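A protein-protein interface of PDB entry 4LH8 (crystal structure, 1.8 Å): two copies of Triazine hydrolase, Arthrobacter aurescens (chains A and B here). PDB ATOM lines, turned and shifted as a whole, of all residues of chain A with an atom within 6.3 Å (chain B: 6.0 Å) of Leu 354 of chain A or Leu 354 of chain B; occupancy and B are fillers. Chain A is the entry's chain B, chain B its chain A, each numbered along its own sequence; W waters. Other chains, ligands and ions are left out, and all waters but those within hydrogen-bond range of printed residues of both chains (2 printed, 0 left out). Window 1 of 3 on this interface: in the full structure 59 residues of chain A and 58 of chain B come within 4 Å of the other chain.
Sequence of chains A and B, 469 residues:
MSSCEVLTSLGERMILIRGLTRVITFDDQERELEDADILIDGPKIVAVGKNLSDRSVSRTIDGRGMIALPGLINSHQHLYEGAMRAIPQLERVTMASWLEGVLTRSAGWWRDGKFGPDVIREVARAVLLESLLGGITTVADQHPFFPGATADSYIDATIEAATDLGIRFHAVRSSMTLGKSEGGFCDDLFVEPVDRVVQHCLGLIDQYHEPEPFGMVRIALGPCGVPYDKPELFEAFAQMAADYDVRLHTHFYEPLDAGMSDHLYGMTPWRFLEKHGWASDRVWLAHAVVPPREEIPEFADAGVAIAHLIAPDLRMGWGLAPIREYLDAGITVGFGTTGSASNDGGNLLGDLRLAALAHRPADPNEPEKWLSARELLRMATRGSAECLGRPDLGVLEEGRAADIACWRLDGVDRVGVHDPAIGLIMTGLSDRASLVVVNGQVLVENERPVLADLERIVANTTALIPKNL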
ATOM      1  N   ILE A 310      18.387  -7.645  -1.497  1.00  0.00           N
ATOM      2  CA  ILE A 310      19.125  -8.644  -0.725  1.00  0.00           C
ATOM      3  C   ILE A 310      20.025  -9.540  -1.576  1.00  0.00           C
ATOM      4  O   ILE A 310      21.159  -9.842  -1.189  1.00  0.00           O
ATOM      5  CB  ILE A 310      18.186  -9.518   0.165  1.00  0.00           C
ATOM      6  CG1 ILE A 310      19.010 -10.430   1.094  1.00  0.00           C
ATOM      7  CG2 ILE A 310      17.212 -10.344  -0.690  1.00  0.00           C
ATOM      8  CD1 ILE A 310      19.738  -9.669   2.213  1.00  0.00           C
ATOM      9  N   ALA A 311      19.531  -9.960  -2.739  1.00  0.00           N
ATOM     10  CA  ALA A 311      20.271 -10.919  -3.551  1.00  0.00           C
ATOM     11  C   ALA A 311      21.644 -10.396  -4.025  1.00  0.00           C
ATOM     12  O   ALA A 311      22.668 -11.047  -3.809  1.00  0.00           O
ATOM     13  CB  ALA A 311      19.412 -11.430  -4.733  1.00  0.00           C
ATOM     14  N   LEU A 314      24.071  -9.803  -0.987  1.00  0.00           N
ATOM     15  CA  LEU A 314      24.738 -11.045  -0.592  1.00  0.00           C
ATOM     16  C   LEU A 314      25.705 -11.538  -1.670  1.00  0.00           C
ATOM     17  O   LEU A 314      26.825 -11.957  -1.367  1.00  0.00           O
ATOM     18  CB  LEU A 314      23.731 -12.148  -0.253  1.00  0.00           C
ATOM     19  CG  LEU A 314      22.718 -11.862   0.858  1.00  0.00           C
ATOM     20  CD1 LEU A 314      21.883 -13.115   1.119  1.00  0.00           C
ATOM     21  CD2 LEU A 314      23.397 -11.369   2.146  1.00  0.00           C
ATOM     22  N   ASN A 343      22.051 -11.785  -9.539  1.00  0.00           N
ATOM     23  CA  ASN A 343      20.936 -12.331  -8.779  1.00  0.00           C
ATOM     24  C   ASN A 343      20.885 -13.862  -8.694  1.00  0.00           C
ATOM     25  O   ASN A 343      20.907 -14.376  -7.580  1.00  0.00           O
ATOM     26  CB  ASN A 343      19.594 -11.749  -9.233  1.00  0.00           C
ATOM     27  CG  ASN A 343      18.445 -12.200  -8.347  1.00  0.00           C
ATOM     28  OD1 ASN A 343      18.136 -13.392  -8.269  1.00  0.00           O
ATOM     29  ND2 ASN A 343      17.817 -11.250  -7.664  1.00  0.00           N
ATOM     30  N   LEU A 349       9.726 -12.932  -5.172  1.00  0.00           N
ATOM     31  CA  LEU A 349       9.169 -13.641  -4.012  1.00  0.00           C
ATOM     32  C   LEU A 349      10.225 -14.554  -3.394  1.00  0.00           C
ATOM     33  O   LEU A 349      10.357 -14.620  -2.178  1.00  0.00           O
ATOM     34  CB  LEU A 349       7.930 -14.449  -4.394  1.00  0.00           C
ATOM     35  CG  LEU A 349       7.353 -15.341  -3.289  1.00  0.00           C
ATOM     36  CD1 LEU A 349       6.984 -14.520  -2.053  1.00  0.00           C
ATOM     37  CD2 LEU A 349       6.133 -16.103  -3.816  1.00  0.00           C
ATOM     38  N   GLY A 350      10.970 -15.263  -4.235  1.00  0.00           N
ATOM     39  CA  GLY A 350      12.049 -16.111  -3.760  1.00  0.00           C
ATOM     40  C   GLY A 350      13.101 -15.331  -2.976  1.00  0.00           C
ATOM     41  O   GLY A 350      13.646 -15.827  -1.986  1.00  0.00           O
ATOM     42  N   ASP A 351      13.406 -14.117  -3.427  1.00  0.00           N
ATOM     43  CA  ASP A 351      14.425 -13.295  -2.754  1.00  0.00           C
ATOM     44  C   ASP A 351      13.973 -12.863  -1.359  1.00  0.00           C
ATOM     45  O   ASP A 351      14.809 -12.605  -0.488  1.00  0.00           O
ATOM     46  CB  ASP A 351      14.795 -12.054  -3.573  1.00  0.00           C
ATOM     47  CG  ASP A 351      15.672 -12.384  -4.769  1.00  0.00           C
ATOM     48  OD1 ASP A 351      16.079 -13.557  -4.913  1.00  0.00           O
ATOM     49  OD2 ASP A 351      15.964 -11.463  -5.556  1.00  0.00           O
ATOM     50  N   LEU A 352      12.659 -12.785  -1.145  1.00  0.00           N
ATOM     51  CA  LEU A 352      12.136 -12.432   0.180  1.00  0.00           C
ATOM     52  C   LEU A 352      12.555 -13.459   1.232  1.00  0.00           C
ATOM     53  O   LEU A 352      12.838 -13.099   2.377  1.00  0.00           O
ATOM     54  CB  LEU A 352      10.603 -12.270   0.173  1.00  0.00           C
ATOM     55  CG  LEU A 352      10.014 -11.149  -0.703  1.00  0.00           C
ATOM     56  CD1 LEU A 352       8.493 -11.114  -0.606  1.00  0.00           C
ATOM     57  CD2 LEU A 352      10.618  -9.784  -0.360  1.00  0.00           C
ATOM     58  N   ARG A 353      12.575 -14.736   0.846  1.00  0.00           N
ATOM     59  CA  ARG A 353      13.046 -15.797   1.735  1.00  0.00           C
ATOM     60  C   ARG A 353      14.515 -15.610   2.101  1.00  0.00           C
ATOM     61  O   ARG A 353      14.913 -15.840   3.240  1.00  0.00           O
ATOM     62  CB  ARG A 353      12.840 -17.179   1.100  1.00  0.00           C
ATOM     63  CG  ARG A 353      13.366 -18.334   1.951  1.00  0.00           C
ATOM     64  CD  ARG A 353      12.902 -19.675   1.393  1.00  0.00           C
ATOM     65  NE  ARG A 353      13.668 -20.808   1.916  1.00  0.00           N
ATOM     66  CZ  ARG A 353      13.511 -21.316   3.133  1.00  0.00           C
ATOM     67  NH1 ARG A 353      14.245 -22.361   3.521  1.00  0.00           N
ATOM     68  NH2 ARG A 353      12.633 -20.771   3.970  1.00  0.00           N
ATOM     69  N   LEU A 354      15.319 -15.192   1.131  1.00  0.00           N
ATOM     70  CA  LEU A 354      16.730 -14.906   1.390  1.00  0.00           C
ATOM     71  C   LEU A 354      16.877 -13.863   2.484  1.00  0.00           C
ATOM     72  O   LEU A 354      17.710 -14.015   3.390  1.00  0.00           O
ATOM     73  CB  LEU A 354      17.441 -14.391   0.132  1.00  0.00           C
ATOM     74  CG  LEU A 354      17.526 -15.244  -1.134  1.00  0.00           C
ATOM     75  CD1 LEU A 354      18.242 -14.459  -2.246  1.00  0.00           C
ATOM     76  CD2 LEU A 354      18.258 -16.543  -0.862  1.00  0.00           C
ATOM     77  N   ALA A 355      16.077 -12.798   2.391  1.00  0.00           N
ATOM     78  CA  ALA A 355      16.129 -11.709   3.363  1.00  0.00           C
ATOM     79  C   ALA A 355      15.587 -12.155   4.722  1.00  0.00           C
ATOM     80  O   ALA A 355      16.141 -11.814   5.765  1.00  0.00           O
ATOM     81  CB  ALA A 355      15.346 -10.490   2.857  1.00  0.00           C
ATOM     82  N   ALA A 356      14.489 -12.903   4.704  1.00  0.00           N
ATOM     83  CA  ALA A 356      13.905 -13.411   5.943  1.00  0.00           C
ATOM     84  C   ALA A 356      14.937 -14.157   6.778  1.00  0.00           C
ATOM     85  O   ALA A 356      14.939 -14.071   8.008  1.00  0.00           O
ATOM     86  CB  ALA A 356      12.706 -14.327   5.641  1.00  0.00           C
ATOM     87  N   LEU A 357      15.806 -14.909   6.115  1.00  0.00           N
ATOM     88  CA  LEU A 357      16.736 -15.763   6.844  1.00  0.00           C
ATOM     89  C   LEU A 357      18.088 -15.095   7.081  1.00  0.00           C
ATOM     90  O   LEU A 357      18.622 -15.154   8.190  1.00  0.00           O
ATOM     91  CB  LEU A 357      16.910 -17.108   6.133  1.00  0.00           C
ATOM     92  CG  LEU A 357      15.639 -17.955   6.064  1.00  0.00           C
ATOM     93  CD1 LEU A 357      15.908 -19.279   5.363  1.00  0.00           C
ATOM     94  CD2 LEU A 357      15.075 -18.180   7.464  1.00  0.00           C
ATOM     95  N   ALA A 358      18.621 -14.433   6.056  1.00  0.00           N
ATOM     96  CA  ALA A 358      19.983 -13.899   6.142  1.00  0.00           C
ATOM     97  C   ALA A 358      20.176 -12.750   7.143  1.00  0.00           C
ATOM     98  O   ALA A 358      21.285 -12.546   7.635  1.00  0.00           O
ATOM     99  CB  ALA A 358      20.511 -13.508   4.756  1.00  0.00           C
ATOM    100  N   HIS A 359      19.119 -12.001   7.445  1.00  0.00           N
ATOM    101  CA  HIS A 359      19.237 -10.911   8.416  1.00  0.00           C
ATOM    102  C   HIS A 359      19.386 -11.391   9.863  1.00  0.00           C
ATOM    103  O   HIS A 359      19.840 -10.640  10.721  1.00  0.00           O
ATOM    104  CB  HIS A 359      18.030  -9.958   8.342  1.00  0.00           C
ATOM    105  CG  HIS A 359      18.123  -8.947   7.245  1.00  0.00           C
ATOM    106  ND1 HIS A 359      18.791  -7.749   7.393  1.00  0.00           N
ATOM    107  CD2 HIS A 359      17.639  -8.955   5.978  1.00  0.00           C
ATOM    108  CE1 HIS A 359      18.716  -7.064   6.264  1.00  0.00           C
ATOM    109  NE2 HIS A 359      18.019  -7.772   5.391  1.00  0.00           N
ATOM    110  N   ILE B 310      22.074 -25.061   6.098  1.00  0.00           N
ATOM    111  CA  ILE B 310      22.070 -23.603   6.044  1.00  0.00           C
ATOM    112  C   ILE B 310      20.754 -22.988   6.531  1.00  0.00           C
ATOM    113  O   ILE B 310      20.769 -21.989   7.261  1.00  0.00           O
ATOM    114  CB  ILE B 310      22.405 -23.085   4.625  1.00  0.00           C
ATOM    115  CG1 ILE B 310      22.568 -21.554   4.631  1.00  0.00           C
ATOM    116  CG2 ILE B 310      21.313 -23.531   3.612  1.00  0.00           C
ATOM    117  CD1 ILE B 310      23.810 -21.047   5.407  1.00  0.00           C
ATOM    118  N   ALA B 311      19.616 -23.569   6.142  1.00  0.00           N
ATOM    119  CA  ALA B 311      18.327 -22.935   6.473  1.00  0.00           C
ATOM    120  C   ALA B 311      18.080 -22.771   7.983  1.00  0.00           C
ATOM    121  O   ALA B 311      17.785 -21.674   8.451  1.00  0.00           O
ATOM    122  CB  ALA B 311      17.149 -23.649   5.785  1.00  0.00           C
ATOM    123  N   LEU B 314      20.570 -20.251   9.691  1.00  0.00           N
ATOM    124  CA  LEU B 314      20.146 -18.872   9.510  1.00  0.00           C
ATOM    125  C   LEU B 314      18.870 -18.572  10.292  1.00  0.00           C
ATOM    126  O   LEU B 314      18.775 -17.544  10.958  1.00  0.00           O
ATOM    127  CB  LEU B 314      19.944 -18.561   8.025  1.00  0.00           C
ATOM    128  CG  LEU B 314      21.165 -18.696   7.114  1.00  0.00           C
ATOM    129  CD1 LEU B 314      20.806 -18.295   5.686  1.00  0.00           C
ATOM    130  CD2 LEU B 314      22.332 -17.856   7.635  1.00  0.00           C
ATOM    131  N   GLY B 350      16.497 -25.679  -3.239  1.00  0.00           N
ATOM    132  CA  GLY B 350      16.322 -24.271  -2.928  1.00  0.00           C
ATOM    133  C   GLY B 350      17.253 -23.789  -1.818  1.00  0.00           C
ATOM    134  O   GLY B 350      17.730 -22.645  -1.833  1.00  0.00           O
ATOM    135  N   ASP B 351      17.503 -24.648  -0.838  1.00  0.00           N
ATOM    136  CA  ASP B 351      18.369 -24.254   0.268  1.00  0.00           C
ATOM    137  C   ASP B 351      19.812 -24.060  -0.211  1.00  0.00           C
ATOM    138  O   ASP B 351      20.580 -23.325   0.408  1.00  0.00           O
ATOM    139  CB  ASP B 351      18.322 -25.264   1.424  1.00  0.00           C
ATOM    140  CG  ASP B 351      17.015 -25.196   2.229  1.00  0.00           C
ATOM    141  OD1 ASP B 351      16.171 -24.308   1.966  1.00  0.00           O
ATOM    142  OD2 ASP B 351      16.848 -26.025   3.149  1.00  0.00           O
ATOM    143  N   LEU B 352      20.180 -24.706  -1.315  1.00  0.00           N
ATOM    144  CA  LEU B 352      21.528 -24.523  -1.866  1.00  0.00           C
ATOM    145  C   LEU B 352      21.794 -23.071  -2.272  1.00  0.00           C
ATOM    146  O   LEU B 352      22.894 -22.570  -2.090  1.00  0.00           O
ATOM    147  CB  LEU B 352      21.798 -25.475  -3.043  1.00  0.00           C
ATOM    148  CG  LEU B 352      21.762 -26.987  -2.749  1.00  0.00           C
ATOM    149  CD1 LEU B 352      22.093 -27.760  -4.009  1.00  0.00           C
ATOM    150  CD2 LEU B 352      22.706 -27.402  -1.613  1.00  0.00           C
ATOM    151  N   ARG B 353      20.787 -22.395  -2.822  1.00  0.00           N
ATOM    152  CA  ARG B 353      20.925 -20.984  -3.189  1.00  0.00           C
ATOM    153  C   ARG B 353      21.172 -20.120  -1.948  1.00  0.00           C
ATOM    154  O   ARG B 353      21.921 -19.145  -1.993  1.00  0.00           O
ATOM    155  CB  ARG B 353      19.675 -20.489  -3.933  1.00  0.00           C
ATOM    156  CG  ARG B 353      19.658 -18.987  -4.246  1.00  0.00           C
ATOM    157  CD  ARG B 353      18.428 -18.603  -5.101  1.00  0.00           C
ATOM    158  NE  ARG B 353      18.160 -17.161  -5.116  1.00  0.00           N
ATOM    159  CZ  ARG B 353      18.848 -16.287  -5.839  1.00  0.00           C
ATOM    160  NH1 ARG B 353      18.539 -14.995  -5.797  1.00  0.00           N
ATOM    161  NH2 ARG B 353      19.861 -16.708  -6.597  1.00  0.00           N
ATOM    162  N   LEU B 354      20.542 -20.494  -0.840  1.00  0.00           N
ATOM    163  CA  LEU B 354      20.739 -19.790   0.425  1.00  0.00           C
ATOM    164  C   LEU B 354      22.199 -19.854   0.836  1.00  0.00           C
ATOM    165  O   LEU B 354      22.783 -18.849   1.252  1.00  0.00           O
ATOM    166  CB  LEU B 354      19.887 -20.412   1.540  1.00  0.00           C
ATOM    167  CG  LEU B 354      18.371 -20.228   1.494  1.00  0.00           C
ATOM    168  CD1 LEU B 354      17.698 -21.022   2.613  1.00  0.00           C
ATOM    169  CD2 LEU B 354      18.033 -18.762   1.620  1.00  0.00           C
ATOM    170  N   ALA B 355      22.780 -21.046   0.741  1.00  0.00           N
ATOM    171  CA  ALA B 355      24.177 -21.231   1.121  1.00  0.00           C
ATOM    172  C   ALA B 355      25.119 -20.528   0.148  1.00  0.00           C
ATOM    173  O   ALA B 355      26.113 -19.920   0.561  1.00  0.00           O
ATOM    174  CB  ALA B 355      24.520 -22.715   1.207  1.00  0.00           C
ATOM    175  N   ALA B 356      24.820 -20.634  -1.145  1.00  0.00           N
ATOM    176  CA  ALA B 356      25.646 -19.982  -2.157  1.00  0.00           C
ATOM    177  C   ALA B 356      25.774 -18.490  -1.884  1.00  0.00           C
ATOM    178  O   ALA B 356      26.835 -17.898  -2.089  1.00  0.00           O
ATOM    179  CB  ALA B 356      25.071 -20.212  -3.548  1.00  0.00           C
ATOM    180  N   LEU B 357      24.685 -17.867  -1.457  1.00  0.00           N
ATOM    181  CA  LEU B 357      24.695 -16.418  -1.280  1.00  0.00           C
ATOM    182  C   LEU B 357      25.099 -16.001   0.135  1.00  0.00           C
ATOM    183  O   LEU B 357      25.888 -15.077   0.311  1.00  0.00           O
ATOM    184  CB  LEU B 357      23.336 -15.812  -1.666  1.00  0.00           C
ATOM    185  CG  LEU B 357      22.972 -15.941  -3.148  1.00  0.00           C
ATOM    186  CD1 LEU B 357      21.613 -15.323  -3.434  1.00  0.00           C
ATOM    187  CD2 LEU B 357      24.038 -15.304  -4.032  1.00  0.00           C
ATOM    188  N   ALA B 358      24.585 -16.698   1.143  1.00  0.00           N
ATOM    189  CA  ALA B 358      24.752 -16.231   2.518  1.00  0.00           C
ATOM    190  C   ALA B 358      26.189 -16.308   3.033  1.00  0.00           C
ATOM    191  O   ALA B 358      26.581 -15.527   3.910  1.00  0.00           O
ATOM    192  CB  ALA B 358      23.797 -16.965   3.465  1.00  0.00           C
ATOM    193  N   HIS B 359      26.980 -17.246   2.515  1.00  0.00           N
ATOM    194  CA  HIS B 359      28.365 -17.377   2.976  1.00  0.00           C
ATOM    195  C   HIS B 359      29.279 -16.242   2.514  1.00  0.00           C
ATOM    196  O   HIS B 359      30.344 -16.039   3.086  1.00  0.00           O
ATOM    197  CB  HIS B 359      28.995 -18.698   2.520  1.00  0.00           C
ATOM    198  CG  HIS B 359      28.586 -19.891   3.329  1.00  0.00           C
ATOM    199  ND1 HIS B 359      29.251 -20.282   4.472  1.00  0.00           N
ATOM    200  CD2 HIS B 359      27.598 -20.798   3.141  1.00  0.00           C
ATOM    201  CE1 HIS B 359      28.682 -21.370   4.962  1.00  0.00           C
ATOM    202  NE2 HIS B 359      27.674 -21.704   4.173  1.00  0.00           N
HETATM  203  O   HOH W   1      15.257 -22.145   0.218  1.00  0.00           O
HETATM  204  O   HOH W   2      15.617 -16.134  -4.082  1.00  0.00           O
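NH1 of Arg 353 of chain A is in salt-bridge range of OD1 of Asp 351 of chain B, 3.1 Å away.
The guanidinium group (NH2) of Arg 353 of chain B is in hydrogen-bond range of the backbone carbonyl oxygen (O) of Asn 343 of chain A (2.7 Å).
The side-chain carboxylate (OD1) of Asp 351 of chain A lies within salt-bridge range of the guanidinium group (NH1) of Arg 353 of chain B (3.0 Å).
OD2 of Asp 351 of chain A sits at hydrogen-bond distance from ND2 of Asn 343 of chain A, 2.8 Å away.
Among the printed residues, pairs that only touch across the chains: Leu 354 of chain A with Leu 354 of chain B (3.3 Å), Leu 354 of chain A with Arg 353 of chain B (3.6 Å), Leu 357 of chain A with Leu 314 of chain B (3.7 Å), Leu 314 of chain A with Leu 357 of chain B (3.7 Å), Leu 354 of chain A with Leu 357 of chain B (3.7 Å), Leu 357 of chain A with Leu 354 of chain B (3.7 Å), Arg 353 of chain A with Leu 354 of chain B (3.8 Å), Ala 311 of chain A with Arg 353 of chain B (3.8 Å) and Arg 353 of chain A with Ala 311 of chain B (3.9 Å).
Of the printed residues of chain B, Asp 351 of chain A touches Arg 353 (3.0 Å).
Of the printed residues of chain B, Arg 353 of chain A touches Ala 311, Asp 351 and Leu 354.
Leu 354 of chain A touches just these residues of chain B: Arg 353, Leu 354 and Leu 357.
His 359 of chain A touches none of the printed residues of chain B.
Of chain A, only Arg 353, Leu 354 and Leu 357 come within 4 Å of Leu 354 of chain B.
Ala 358 of chain B touches none of the printed residues of chain A.
The nearest printed residue of chain A that does not touch Leu 357 of chain B is Asn 343 of chain A (4.3 Å).
Of the 13 printed residues of chain B, 6 touch a printed residue of chain A.
Printed residues of chain B that touch a printed residue of chain A: Ala 311, Leu 314, Asp 351, Arg 353, Leu 354 and Leu 357.
Hydrophobic or aromatic side chains of chain B that line the printed part of chain A: Ala 311, Leu 314, Leu 354 and Leu 357.
Hydrophobic or aromatic side chains of chain A that line the printed part of chain B: Ala 311, Leu 314, Leu 354 and Leu 357.
Among the printed residues, Asp or Glu carboxylates within 4 Å of a Lys or Arg side-chain nitrogen of the other chain: Asp 351 of chain A with Arg 353 of chain B (3.0 Å) and Arg 353 of chain A with Asp 351 of chain B (3.1 Å).
Ala 311 of chain A touches Arg 353 of chain B, and with the chains exchanged Arg 353 of chain A touches Ala 311 of chain B.
Leu 314 of chain A touches Leu 357 of chain B, and with the chains exchanged Leu 357 of chain A touches Leu 314 of chain B.
Leu 354 of chain A touches its own counterpart, Leu 354 of chain B.
Leu 354 of chain A touches Leu 357 of chain B, and with the chains exchanged Leu 357 of chain A touches Leu 354 of chain B.
Water W1 lies within hydrogen-bond range of NE of Arg 353 of chain A (2.7 Å), OD1 of Asp 351 of chain B (2.9 Å) and O of Gly 350 of chain B (3.3 Å).
Water W2 lies within hydrogen-bond range of the side-chain carboxylate (OD1) of Asp 351 of chain A, the backbone carbonyl oxygen (O) of Gly 350 of chain A and the guanidinium group (NE) of Arg 353 of chain B.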
